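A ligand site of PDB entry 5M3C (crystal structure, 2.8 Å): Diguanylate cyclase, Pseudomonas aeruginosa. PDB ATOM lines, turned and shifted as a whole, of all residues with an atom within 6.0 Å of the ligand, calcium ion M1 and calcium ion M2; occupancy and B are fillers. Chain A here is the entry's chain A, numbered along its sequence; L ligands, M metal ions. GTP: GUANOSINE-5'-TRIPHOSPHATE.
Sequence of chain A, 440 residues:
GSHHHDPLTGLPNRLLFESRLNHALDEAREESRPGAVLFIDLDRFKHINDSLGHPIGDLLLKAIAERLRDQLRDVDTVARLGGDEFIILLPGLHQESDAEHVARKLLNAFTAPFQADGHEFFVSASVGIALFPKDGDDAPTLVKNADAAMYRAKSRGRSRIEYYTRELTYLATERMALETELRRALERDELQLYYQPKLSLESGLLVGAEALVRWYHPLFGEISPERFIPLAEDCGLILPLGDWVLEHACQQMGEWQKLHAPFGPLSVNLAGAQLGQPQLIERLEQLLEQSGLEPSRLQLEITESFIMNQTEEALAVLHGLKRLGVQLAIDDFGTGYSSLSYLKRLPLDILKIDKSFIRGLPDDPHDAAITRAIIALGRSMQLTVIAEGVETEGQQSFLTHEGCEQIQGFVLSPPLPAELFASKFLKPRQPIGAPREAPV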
ATOM      1  N   LEU A   8     -22.680 -25.046   2.427  1.00  0.00           N
ATOM      2  CA  LEU A   8     -21.694 -24.382   3.258  1.00  0.00           C
ATOM      3  C   LEU A   8     -20.864 -25.358   4.087  1.00  0.00           C
ATOM      4  O   LEU A   8     -19.633 -25.265   4.139  1.00  0.00           O
ATOM      5  CB  LEU A   8     -22.370 -23.364   4.177  1.00  0.00           C
ATOM      6  CG  LEU A   8     -21.502 -22.745   5.283  1.00  0.00           C
ATOM      7  CD1 LEU A   8     -20.203 -22.173   4.727  1.00  0.00           C
ATOM      8  CD2 LEU A   8     -22.289 -21.676   6.024  1.00  0.00           C
ATOM      9  N   ASP A  41     -27.744 -25.510  19.385  1.00  0.00           N
ATOM     10  CA  ASP A  41     -27.846 -24.143  18.898  1.00  0.00           C
ATOM     11  C   ASP A  41     -26.712 -23.329  19.508  1.00  0.00           C
ATOM     12  O   ASP A  41     -26.425 -23.448  20.700  1.00  0.00           O
ATOM     13  CB  ASP A  41     -29.209 -23.548  19.280  1.00  0.00           C
ATOM     14  CG  ASP A  41     -29.340 -22.099  18.886  1.00  0.00           C
ATOM     15  OD1 ASP A  41     -28.698 -21.244  19.522  1.00  0.00           O
ATOM     16  OD2 ASP A  41     -30.107 -21.808  17.949  1.00  0.00           O
ATOM     17  N   LEU A  42     -26.066 -22.508  18.694  1.00  0.00           N
ATOM     18  CA  LEU A  42     -24.891 -21.773  19.118  1.00  0.00           C
ATOM     19  C   LEU A  42     -25.235 -20.612  20.040  1.00  0.00           C
ATOM     20  O   LEU A  42     -26.262 -19.950  19.871  1.00  0.00           O
ATOM     21  CB  LEU A  42     -24.105 -21.252  17.899  1.00  0.00           C
ATOM     22  CG  LEU A  42     -23.623 -22.321  16.917  1.00  0.00           C
ATOM     23  CD1 LEU A  42     -23.060 -21.667  15.668  1.00  0.00           C
ATOM     24  CD2 LEU A  42     -22.590 -23.241  17.551  1.00  0.00           C
ATOM     25  N   ASP A  43     -24.370 -20.365  21.028  1.00  0.00           N
ATOM     26  CA  ASP A  43     -24.592 -19.309  22.007  1.00  0.00           C
ATOM     27  C   ASP A  43     -24.222 -17.940  21.451  1.00  0.00           C
ATOM     28  O   ASP A  43     -23.097 -17.718  21.011  1.00  0.00           O
ATOM     29  CB  ASP A  43     -23.804 -19.590  23.287  1.00  0.00           C
ATOM     30  CG  ASP A  43     -24.419 -20.699  24.129  1.00  0.00           C
ATOM     31  OD1 ASP A  43     -25.572 -21.081  23.869  1.00  0.00           O
ATOM     32  OD2 ASP A  43     -23.740 -21.184  25.065  1.00  0.00           O
ATOM     33  N   ARG A  44     -25.194 -17.037  21.489  1.00  0.00           N
ATOM     34  CA  ARG A  44     -25.026 -15.651  21.037  1.00  0.00           C
ATOM     35  C   ARG A  44     -24.164 -15.527  19.779  1.00  0.00           C
ATOM     36  O   ARG A  44     -23.019 -15.091  19.843  1.00  0.00           O
ATOM     37  CB  ARG A  44     -24.457 -14.805  22.181  1.00  0.00           C
ATOM     38  CG  ARG A  44     -25.422 -14.649  23.339  1.00  0.00           C
ATOM     39  CD  ARG A  44     -24.714 -14.258  24.634  1.00  0.00           C
ATOM     40  N   PHE A  45     -24.752 -15.905  18.644  1.00  0.00           N
ATOM     41  CA  PHE A  45     -24.036 -15.912  17.366  1.00  0.00           C
ATOM     42  C   PHE A  45     -24.235 -14.616  16.564  1.00  0.00           C
ATOM     43  O   PHE A  45     -23.376 -14.267  15.757  1.00  0.00           O
ATOM     44  CB  PHE A  45     -24.461 -17.113  16.530  1.00  0.00           C
ATOM     45  CG  PHE A  45     -23.412 -17.573  15.561  1.00  0.00           C
ATOM     46  CD1 PHE A  45     -22.183 -18.011  16.023  1.00  0.00           C
ATOM     47  CD2 PHE A  45     -23.641 -17.562  14.196  1.00  0.00           C
ATOM     48  CE1 PHE A  45     -21.205 -18.431  15.153  1.00  0.00           C
ATOM     49  CE2 PHE A  45     -22.663 -17.984  13.312  1.00  0.00           C
ATOM     50  CZ  PHE A  45     -21.446 -18.421  13.794  1.00  0.00           C
ATOM     51  N   LYS A  46     -25.351 -13.935  16.777  1.00  0.00           N
ATOM     52  CA  LYS A  46     -25.594 -12.657  16.084  1.00  0.00           C
ATOM     53  C   LYS A  46     -24.483 -11.676  16.415  1.00  0.00           C
ATOM     54  O   LYS A  46     -23.872 -11.071  15.520  1.00  0.00           O
ATOM     55  CB  LYS A  46     -26.951 -12.072  16.476  1.00  0.00           C
ATOM     56  N   HIS A  47     -24.195 -11.528  17.706  1.00  0.00           N
ATOM     57  CA  HIS A  47     -23.135 -10.641  18.194  1.00  0.00           C
ATOM     58  C   HIS A  47     -21.808 -10.933  17.502  1.00  0.00           C
ATOM     59  O   HIS A  47     -20.986 -10.031  17.320  1.00  0.00           O
ATOM     60  CB  HIS A  47     -22.962 -10.786  19.702  1.00  0.00           C
ATOM     61  N   ASN A  49     -21.668 -12.365  14.344  1.00  0.00           N
ATOM     62  CA  ASN A  49     -21.865 -11.979  12.947  1.00  0.00           C
ATOM     63  C   ASN A  49     -21.726 -10.468  12.768  1.00  0.00           C
ATOM     64  O   ASN A  49     -21.200 -10.006  11.757  1.00  0.00           O
ATOM     65  CB  ASN A  49     -23.241 -12.426  12.439  1.00  0.00           C
ATOM     66  CG  ASN A  49     -23.187 -13.777  11.753  1.00  0.00           C
ATOM     67  OD1 ASN A  49     -22.248 -14.553  11.937  1.00  0.00           O
ATOM     68  ND2 ASN A  49     -24.216 -14.068  10.960  1.00  0.00           N
ATOM     69  N   GLY A  53     -18.433 -10.152  11.338  1.00  0.00           N
ATOM     70  CA  GLY A  53     -18.902 -10.212   9.954  1.00  0.00           C
ATOM     71  C   GLY A  53     -19.062 -11.627   9.428  1.00  0.00           C
ATOM     72  O   GLY A  53     -18.360 -12.545   9.863  1.00  0.00           O
ATOM     73  N   HIS A  54     -19.974 -11.798   8.483  1.00  0.00           N
ATOM     74  CA  HIS A  54     -20.252 -13.106   7.878  1.00  0.00           C
ATOM     75  C   HIS A  54     -18.989 -13.908   7.533  1.00  0.00           C
ATOM     76  O   HIS A  54     -18.931 -15.112   7.806  1.00  0.00           O
ATOM     77  CB  HIS A  54     -21.110 -12.947   6.616  1.00  0.00           C
ATOM     78  CG  HIS A  54     -22.536 -13.378   6.806  1.00  0.00           C
ATOM     79  ND1 HIS A  54     -23.076 -14.450   6.146  1.00  0.00           N
ATOM     80  CD2 HIS A  54     -23.517 -12.868   7.583  1.00  0.00           C
ATOM     81  CE1 HIS A  54     -24.343 -14.593   6.503  1.00  0.00           C
ATOM     82  NE2 HIS A  54     -24.636 -13.646   7.368  1.00  0.00           N
ATOM     83  N   PRO A  55     -17.993 -13.267   6.898  1.00  0.00           N
ATOM     84  CA  PRO A  55     -16.746 -13.954   6.584  1.00  0.00           C
ATOM     85  C   PRO A  55     -16.313 -14.905   7.696  1.00  0.00           C
ATOM     86  O   PRO A  55     -16.086 -16.085   7.447  1.00  0.00           O
ATOM     87  CB  PRO A  55     -15.746 -12.801   6.438  1.00  0.00           C
ATOM     88  CG  PRO A  55     -16.569 -11.587   6.121  1.00  0.00           C
ATOM     89  CD  PRO A  55     -18.023 -11.906   6.335  1.00  0.00           C
ATOM     90  N   ILE A  56     -16.188 -14.383   8.912  1.00  0.00           N
ATOM     91  CA  ILE A  56     -15.787 -15.179  10.062  1.00  0.00           C
ATOM     92  C   ILE A  56     -16.861 -16.206  10.400  1.00  0.00           C
ATOM     93  O   ILE A  56     -16.567 -17.381  10.662  1.00  0.00           O
ATOM     94  CB  ILE A  56     -15.519 -14.295  11.296  1.00  0.00           C
ATOM     95  CG1 ILE A  56     -14.434 -13.260  10.993  1.00  0.00           C
ATOM     96  CG2 ILE A  56     -15.129 -15.150  12.491  1.00  0.00           C
ATOM     97  CD1 ILE A  56     -13.076 -13.853  10.660  1.00  0.00           C
ATOM     98  N   GLY A  57     -18.118 -15.766  10.396  1.00  0.00           N
ATOM     99  CA  GLY A  57     -19.249 -16.639  10.684  1.00  0.00           C
ATOM    100  C   GLY A  57     -19.256 -17.896   9.844  1.00  0.00           C
ATOM    101  O   GLY A  57     -19.045 -18.995  10.363  1.00  0.00           O
ATOM    102  N   ASP A  58     -19.494 -17.746   8.542  1.00  0.00           N
ATOM    103  CA  ASP A  58     -19.560 -18.884   7.629  1.00  0.00           C
ATOM    104  C   ASP A  58     -18.400 -19.849   7.831  1.00  0.00           C
ATOM    105  O   ASP A  58     -18.542 -21.053   7.616  1.00  0.00           O
ATOM    106  CB  ASP A  58     -19.592 -18.397   6.164  1.00  0.00           C
ATOM    107  CG  ASP A  58     -20.936 -17.832   5.763  1.00  0.00           C
ATOM    108  OD1 ASP A  58     -21.546 -17.105   6.582  1.00  0.00           O
ATOM    109  OD2 ASP A  58     -21.383 -18.094   4.635  1.00  0.00           O
ATOM    110  N   LEU A  61     -18.783 -21.842  11.351  1.00  0.00           N
ATOM    111  CA  LEU A  61     -19.754 -22.916  11.169  1.00  0.00           C
ATOM    112  C   LEU A  61     -19.091 -24.151  10.558  1.00  0.00           C
ATOM    113  O   LEU A  61     -19.323 -25.270  11.007  1.00  0.00           O
ATOM    114  CB  LEU A  61     -20.923 -22.448  10.296  1.00  0.00           C
ATOM    115  CG  LEU A  61     -21.817 -21.358  10.894  1.00  0.00           C
ATOM    116  CD1 LEU A  61     -22.803 -20.843   9.862  1.00  0.00           C
ATOM    117  CD2 LEU A  61     -22.540 -21.859  12.126  1.00  0.00           C
ATOM    118  N   ARG A  80     -26.967 -29.964   9.627  1.00  0.00           N
ATOM    119  CA  ARG A  80     -27.288 -28.560   9.857  1.00  0.00           C
ATOM    120  C   ARG A  80     -28.739 -28.367   9.485  1.00  0.00           C
ATOM    121  O   ARG A  80     -29.153 -28.696   8.377  1.00  0.00           O
ATOM    122  CB  ARG A  80     -26.403 -27.637   9.006  1.00  0.00           C
ATOM    123  CG  ARG A  80     -26.281 -26.223   9.567  1.00  0.00           C
ATOM    124  CD  ARG A  80     -25.404 -25.322   8.698  1.00  0.00           C
ATOM    125  NE  ARG A  80     -26.196 -24.440   7.835  1.00  0.00           N
ATOM    126  CZ  ARG A  80     -26.226 -23.108   7.937  1.00  0.00           C
ATOM    127  NH1 ARG A  80     -26.967 -22.397   7.097  1.00  0.00           N
ATOM    128  NH2 ARG A  80     -25.511 -22.483   8.857  1.00  0.00           N
ATOM    129  N   GLY A  82     -30.359 -25.570   9.345  1.00  0.00           N
ATOM    130  CA  GLY A  82     -30.599 -24.202   8.903  1.00  0.00           C
ATOM    131  C   GLY A  82     -30.280 -23.255  10.035  1.00  0.00           C
ATOM    132  O   GLY A  82     -30.465 -23.586  11.209  1.00  0.00           O
ATOM    133  N   GLY A  83     -29.795 -22.068   9.685  1.00  0.00           N
ATOM    134  CA  GLY A  83     -29.357 -21.108  10.697  1.00  0.00           C
ATOM    135  C   GLY A  83     -28.146 -21.639  11.432  1.00  0.00           C
ATOM    136  O   GLY A  83     -27.350 -22.399  10.884  1.00  0.00           O
ATOM    137  N   ASP A  84     -27.994 -21.242  12.692  1.00  0.00           N
ATOM    138  CA  ASP A  84     -26.856 -21.672  13.500  1.00  0.00           C
ATOM    139  C   ASP A  84     -27.235 -22.895  14.326  1.00  0.00           C
ATOM    140  O   ASP A  84     -26.939 -22.946  15.528  1.00  0.00           O
ATOM    141  CB  ASP A  84     -26.401 -20.552  14.422  1.00  0.00           C
ATOM    142  CG  ASP A  84     -27.428 -20.215  15.483  1.00  0.00           C
ATOM    143  OD1 ASP A  84     -28.608 -20.586  15.322  1.00  0.00           O
ATOM    144  OD2 ASP A  84     -27.057 -19.572  16.488  1.00  0.00           O
ATOM    145  N   GLU A  85     -27.870 -23.878  13.697  1.00  0.00           N
ATOM    146  CA  GLU A  85     -28.453 -24.995  14.419  1.00  0.00           C
ATOM    147  C   GLU A  85     -28.077 -26.346  13.816  1.00  0.00           C
ATOM    148  O   GLU A  85     -28.317 -26.603  12.638  1.00  0.00           O
ATOM    149  CB  GLU A  85     -29.968 -24.834  14.480  1.00  0.00           C
ATOM    150  CG  GLU A  85     -30.421 -23.642  15.314  1.00  0.00           C
ATOM    151  CD  GLU A  85     -31.896 -23.304  15.154  1.00  0.00           C
ATOM    152  OE1 GLU A  85     -32.588 -23.969  14.356  1.00  0.00           O
ATOM    153  OE2 GLU A  85     -32.352 -22.369  15.844  1.00  0.00           O
ATOM    154  N   LYS A 154     -30.897 -22.554  27.229  1.00  0.00           N
ATOM    155  CA  LYS A 154     -30.835 -21.101  27.107  1.00  0.00           C
ATOM    156  C   LYS A 154     -31.427 -20.468  28.365  1.00  0.00           C
ATOM    157  O   LYS A 154     -30.888 -19.499  28.906  1.00  0.00           O
ATOM    158  CB  LYS A 154     -31.639 -20.619  25.901  1.00  0.00           C
ATOM    159  CG  LYS A 154     -31.115 -21.106  24.559  1.00  0.00           C
ATOM    160  CD  LYS A 154     -29.688 -20.635  24.319  1.00  0.00           C
ATOM    161  CE  LYS A 154     -29.300 -20.821  22.865  1.00  0.00           C
ATOM    162  NZ  LYS A 154     -27.822 -20.751  22.700  1.00  0.00           N
ATOM    163  N   ARG A 158     -26.358 -20.531  30.053  1.00  0.00           N
ATOM    164  CA  ARG A 158     -26.044 -21.020  28.711  1.00  0.00           C
ATOM    165  C   ARG A 158     -24.890 -22.013  28.752  1.00  0.00           C
ATOM    166  O   ARG A 158     -24.441 -22.408  29.831  1.00  0.00           O
ATOM    167  CB  ARG A 158     -25.713 -19.853  27.778  1.00  0.00           C
ATOM    168  CG  ARG A 158     -26.930 -19.245  27.117  1.00  0.00           C
ATOM    169  CD  ARG A 158     -26.575 -18.029  26.277  1.00  0.00           C
ATOM    170  NE  ARG A 158     -27.730 -17.488  25.572  1.00  0.00           N
ATOM    171  CZ  ARG A 158     -28.771 -16.891  26.152  1.00  0.00           C
ATOM    172  NH1 ARG A 158     -29.773 -16.435  25.416  1.00  0.00           N
ATOM    173  NH2 ARG A 158     -28.816 -16.762  27.470  1.00  0.00           N
ATOM    174  N   ASP A 234     -32.588 -10.415  24.579  1.00  0.00           N
ATOM    175  CA  ASP A 234     -33.006 -11.158  23.388  1.00  0.00           C
ATOM    176  C   ASP A 234     -33.809 -10.303  22.414  1.00  0.00           C
ATOM    177  O   ASP A 234     -33.605 -10.374  21.200  1.00  0.00           O
ATOM    178  CB  ASP A 234     -33.809 -12.398  23.799  1.00  0.00           C
ATOM    179  CG  ASP A 234     -32.955 -13.415  24.536  1.00  0.00           C
ATOM    180  OD1 ASP A 234     -31.790 -13.626  24.133  1.00  0.00           O
ATOM    181  OD2 ASP A 234     -33.448 -14.006  25.526  1.00  0.00           O
HETATM  182  PG  GTP L   1     -28.959 -17.112  21.413  1.00  0.00           P
HETATM  183  O1G GTP L   1     -28.137 -17.304  22.665  1.00  0.00           O
HETATM  184  O2G GTP L   1     -28.977 -18.334  20.516  1.00  0.00           O
HETATM  185  O3G GTP L   1     -30.314 -16.487  21.654  1.00  0.00           O
HETATM  186  O3B GTP L   1     -28.145 -16.005  20.565  1.00  0.00           O
HETATM  187  PB  GTP L   1     -28.202 -15.945  18.961  1.00  0.00           P
HETATM  188  O1B GTP L   1     -27.678 -14.601  18.515  1.00  0.00           O
HETATM  189  O2B GTP L   1     -27.563 -17.192  18.408  1.00  0.00           O
HETATM  190  O3A GTP L   1     -29.781 -15.991  18.645  1.00  0.00           O
HETATM  191  PA  GTP L   1     -30.317 -16.669  17.296  1.00  0.00           P
HETATM  192  O1A GTP L   1     -31.648 -16.063  16.953  1.00  0.00           O
HETATM  193  O2A GTP L   1     -30.163 -18.166  17.390  1.00  0.00           O
HETATM  194  O5' GTP L   1     -29.244 -16.134  16.243  1.00  0.00           O
HETATM  195  C5' GTP L   1     -29.165 -16.732  14.960  1.00  0.00           C
HETATM  196  C4' GTP L   1     -28.024 -16.038  14.243  1.00  0.00           C
HETATM  197  O4' GTP L   1     -27.266 -16.963  13.469  1.00  0.00           O
HETATM  198  C3' GTP L   1     -28.567 -14.968  13.315  1.00  0.00           C
HETATM  199  O3' GTP L   1     -27.955 -13.707  13.610  1.00  0.00           O
HETATM  200  C2' GTP L   1     -28.180 -15.451  11.931  1.00  0.00           C
HETATM  201  O2' GTP L   1     -27.835 -14.386  11.051  1.00  0.00           O
HETATM  202  C1' GTP L   1     -26.987 -16.348  12.216  1.00  0.00           C
HETATM  203  N9  GTP L   1     -26.829 -17.291  11.094  1.00  0.00           N
HETATM  204  C8  GTP L   1     -27.731 -18.185  10.641  1.00  0.00           C
HETATM  205  N7  GTP L   1     -27.233 -18.856   9.573  1.00  0.00           N
HETATM  206  C5  GTP L   1     -25.990 -18.378   9.325  1.00  0.00           C
HETATM  207  C6  GTP L   1     -24.913 -18.631   8.352  1.00  0.00           C
HETATM  208  O6  GTP L   1     -25.048 -19.502   7.472  1.00  0.00           O
HETATM  209  N1  GTP L   1     -23.783 -17.907   8.446  1.00  0.00           N
HETATM  210  C2  GTP L   1     -23.612 -16.963   9.401  1.00  0.00           C
HETATM  211  N2  GTP L   1     -22.447 -16.272   9.438  1.00  0.00           N
HETATM  212  N3  GTP L   1     -24.558 -16.677  10.323  1.00  0.00           N
HETATM  213  C4  GTP L   1     -25.740 -17.345  10.333  1.00  0.00           C
HETATM  214 CA    CA M   1     -28.215 -19.464  18.472  1.00  0.00          CA
HETATM  215 CA    CA M   2     -31.060 -20.245  15.986  1.00  0.00          CA
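OD1 of Asp 41 sits close to NZ of Lys 154 (3.3 Å). O of Leu 42 lies close to NZ of Lys 154 (3.3 Å). The guanidinium group (NH1) of Arg 158 is in salt-bridge range of the side-chain carboxylate (OD1) of Asp 234 (3.7 Å). A ring nitrogen (ND1) of His 54 lies within hydrogen-bond range of the side-chain carboxylate (OD1) of Asp 58, 3.1 Å away. The backbone carbonyl oxygen (O) of Gly 83 is in hydrogen-bond range of the guanidinium group (NH2) of Arg 80, 2.7 Å away. The side-chain amino group of Lys 154 is in salt-bridge range of the side-chain carboxylate of Asp 43 (2.6 Å).
N3 of the ligand is in hydrogen-bond range of ND2 of Asn 49 (2.7 Å). NE of Arg 158 lies within salt-bridge range of O1G of the ligand. N of Lys 46 is in hydrogen-bond range of O1B of the ligand, at 3.0 Å. The side-chain carboxylate (OD1) of Asp 58 sits at hydrogen-bond distance from a nitrogen (N1) of the ligand (3.0 Å). An oxygen (O1B) of the ligand sits at hydrogen-bond distance from the backbone NH (N) of Phe 45, at 3.2 Å. N of Arg 44 sits at hydrogen-bond distance from O1G of the ligand. NH2 of Arg 80 is in hydrogen-bond range of O6 of the ligand (3.3 Å). O1G of the ligand lies within salt-bridge range of NZ of Lys 154 (3.5 Å).
CD2 of Leu 8 touches O6 of the ligand (3.8 Å). His 54 touches the ligand (CE1 to C2, 3.8 Å). CA of Gly 57 touches N2 of the ligand (3.5 Å). Leu 61 touches the ligand (CD1 to N1, 3.4 Å). Gly 83 touches the ligand. Hydrophobic or aromatic side chains that line the ligand: Leu 8, Phe 45, His 54 and Leu 61. Within 4 Å of the ligand: Leu 8, Asp 41, Leu 42, Arg 44, Phe 45, Lys 46, Asn 49, His 54, Gly 57, Asp 58, Leu 61, Arg 80, Gly 83, Asp 84, Lys 154 and Arg 158.
Calcium ion M2 is bound by OE2 of Glu 85 (2.5 Å), OD1 of Asp 84 (2.6 Å), O2A of the ligand (2.7 Å) and OD2 of Asp 41 (2.7 Å).
Calcium ion M1 is bound by OD1 of Asp 41, OD2 of Asp 84, O2B of the ligand, O of Leu 42, O2G of the ligand and O2A of the ligand. Slightly farther from calcium ion M1 lies the side-chain carboxylate (OD2) of Asp 41 (3.1 Å).
Three residues have an atom within 4 Å of calcium ion M1: Asp 41, Leu 42 and Asp 84. The nearest printed residue that does not touch calcium ion M1 is Lys 154 (4.4 Å).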
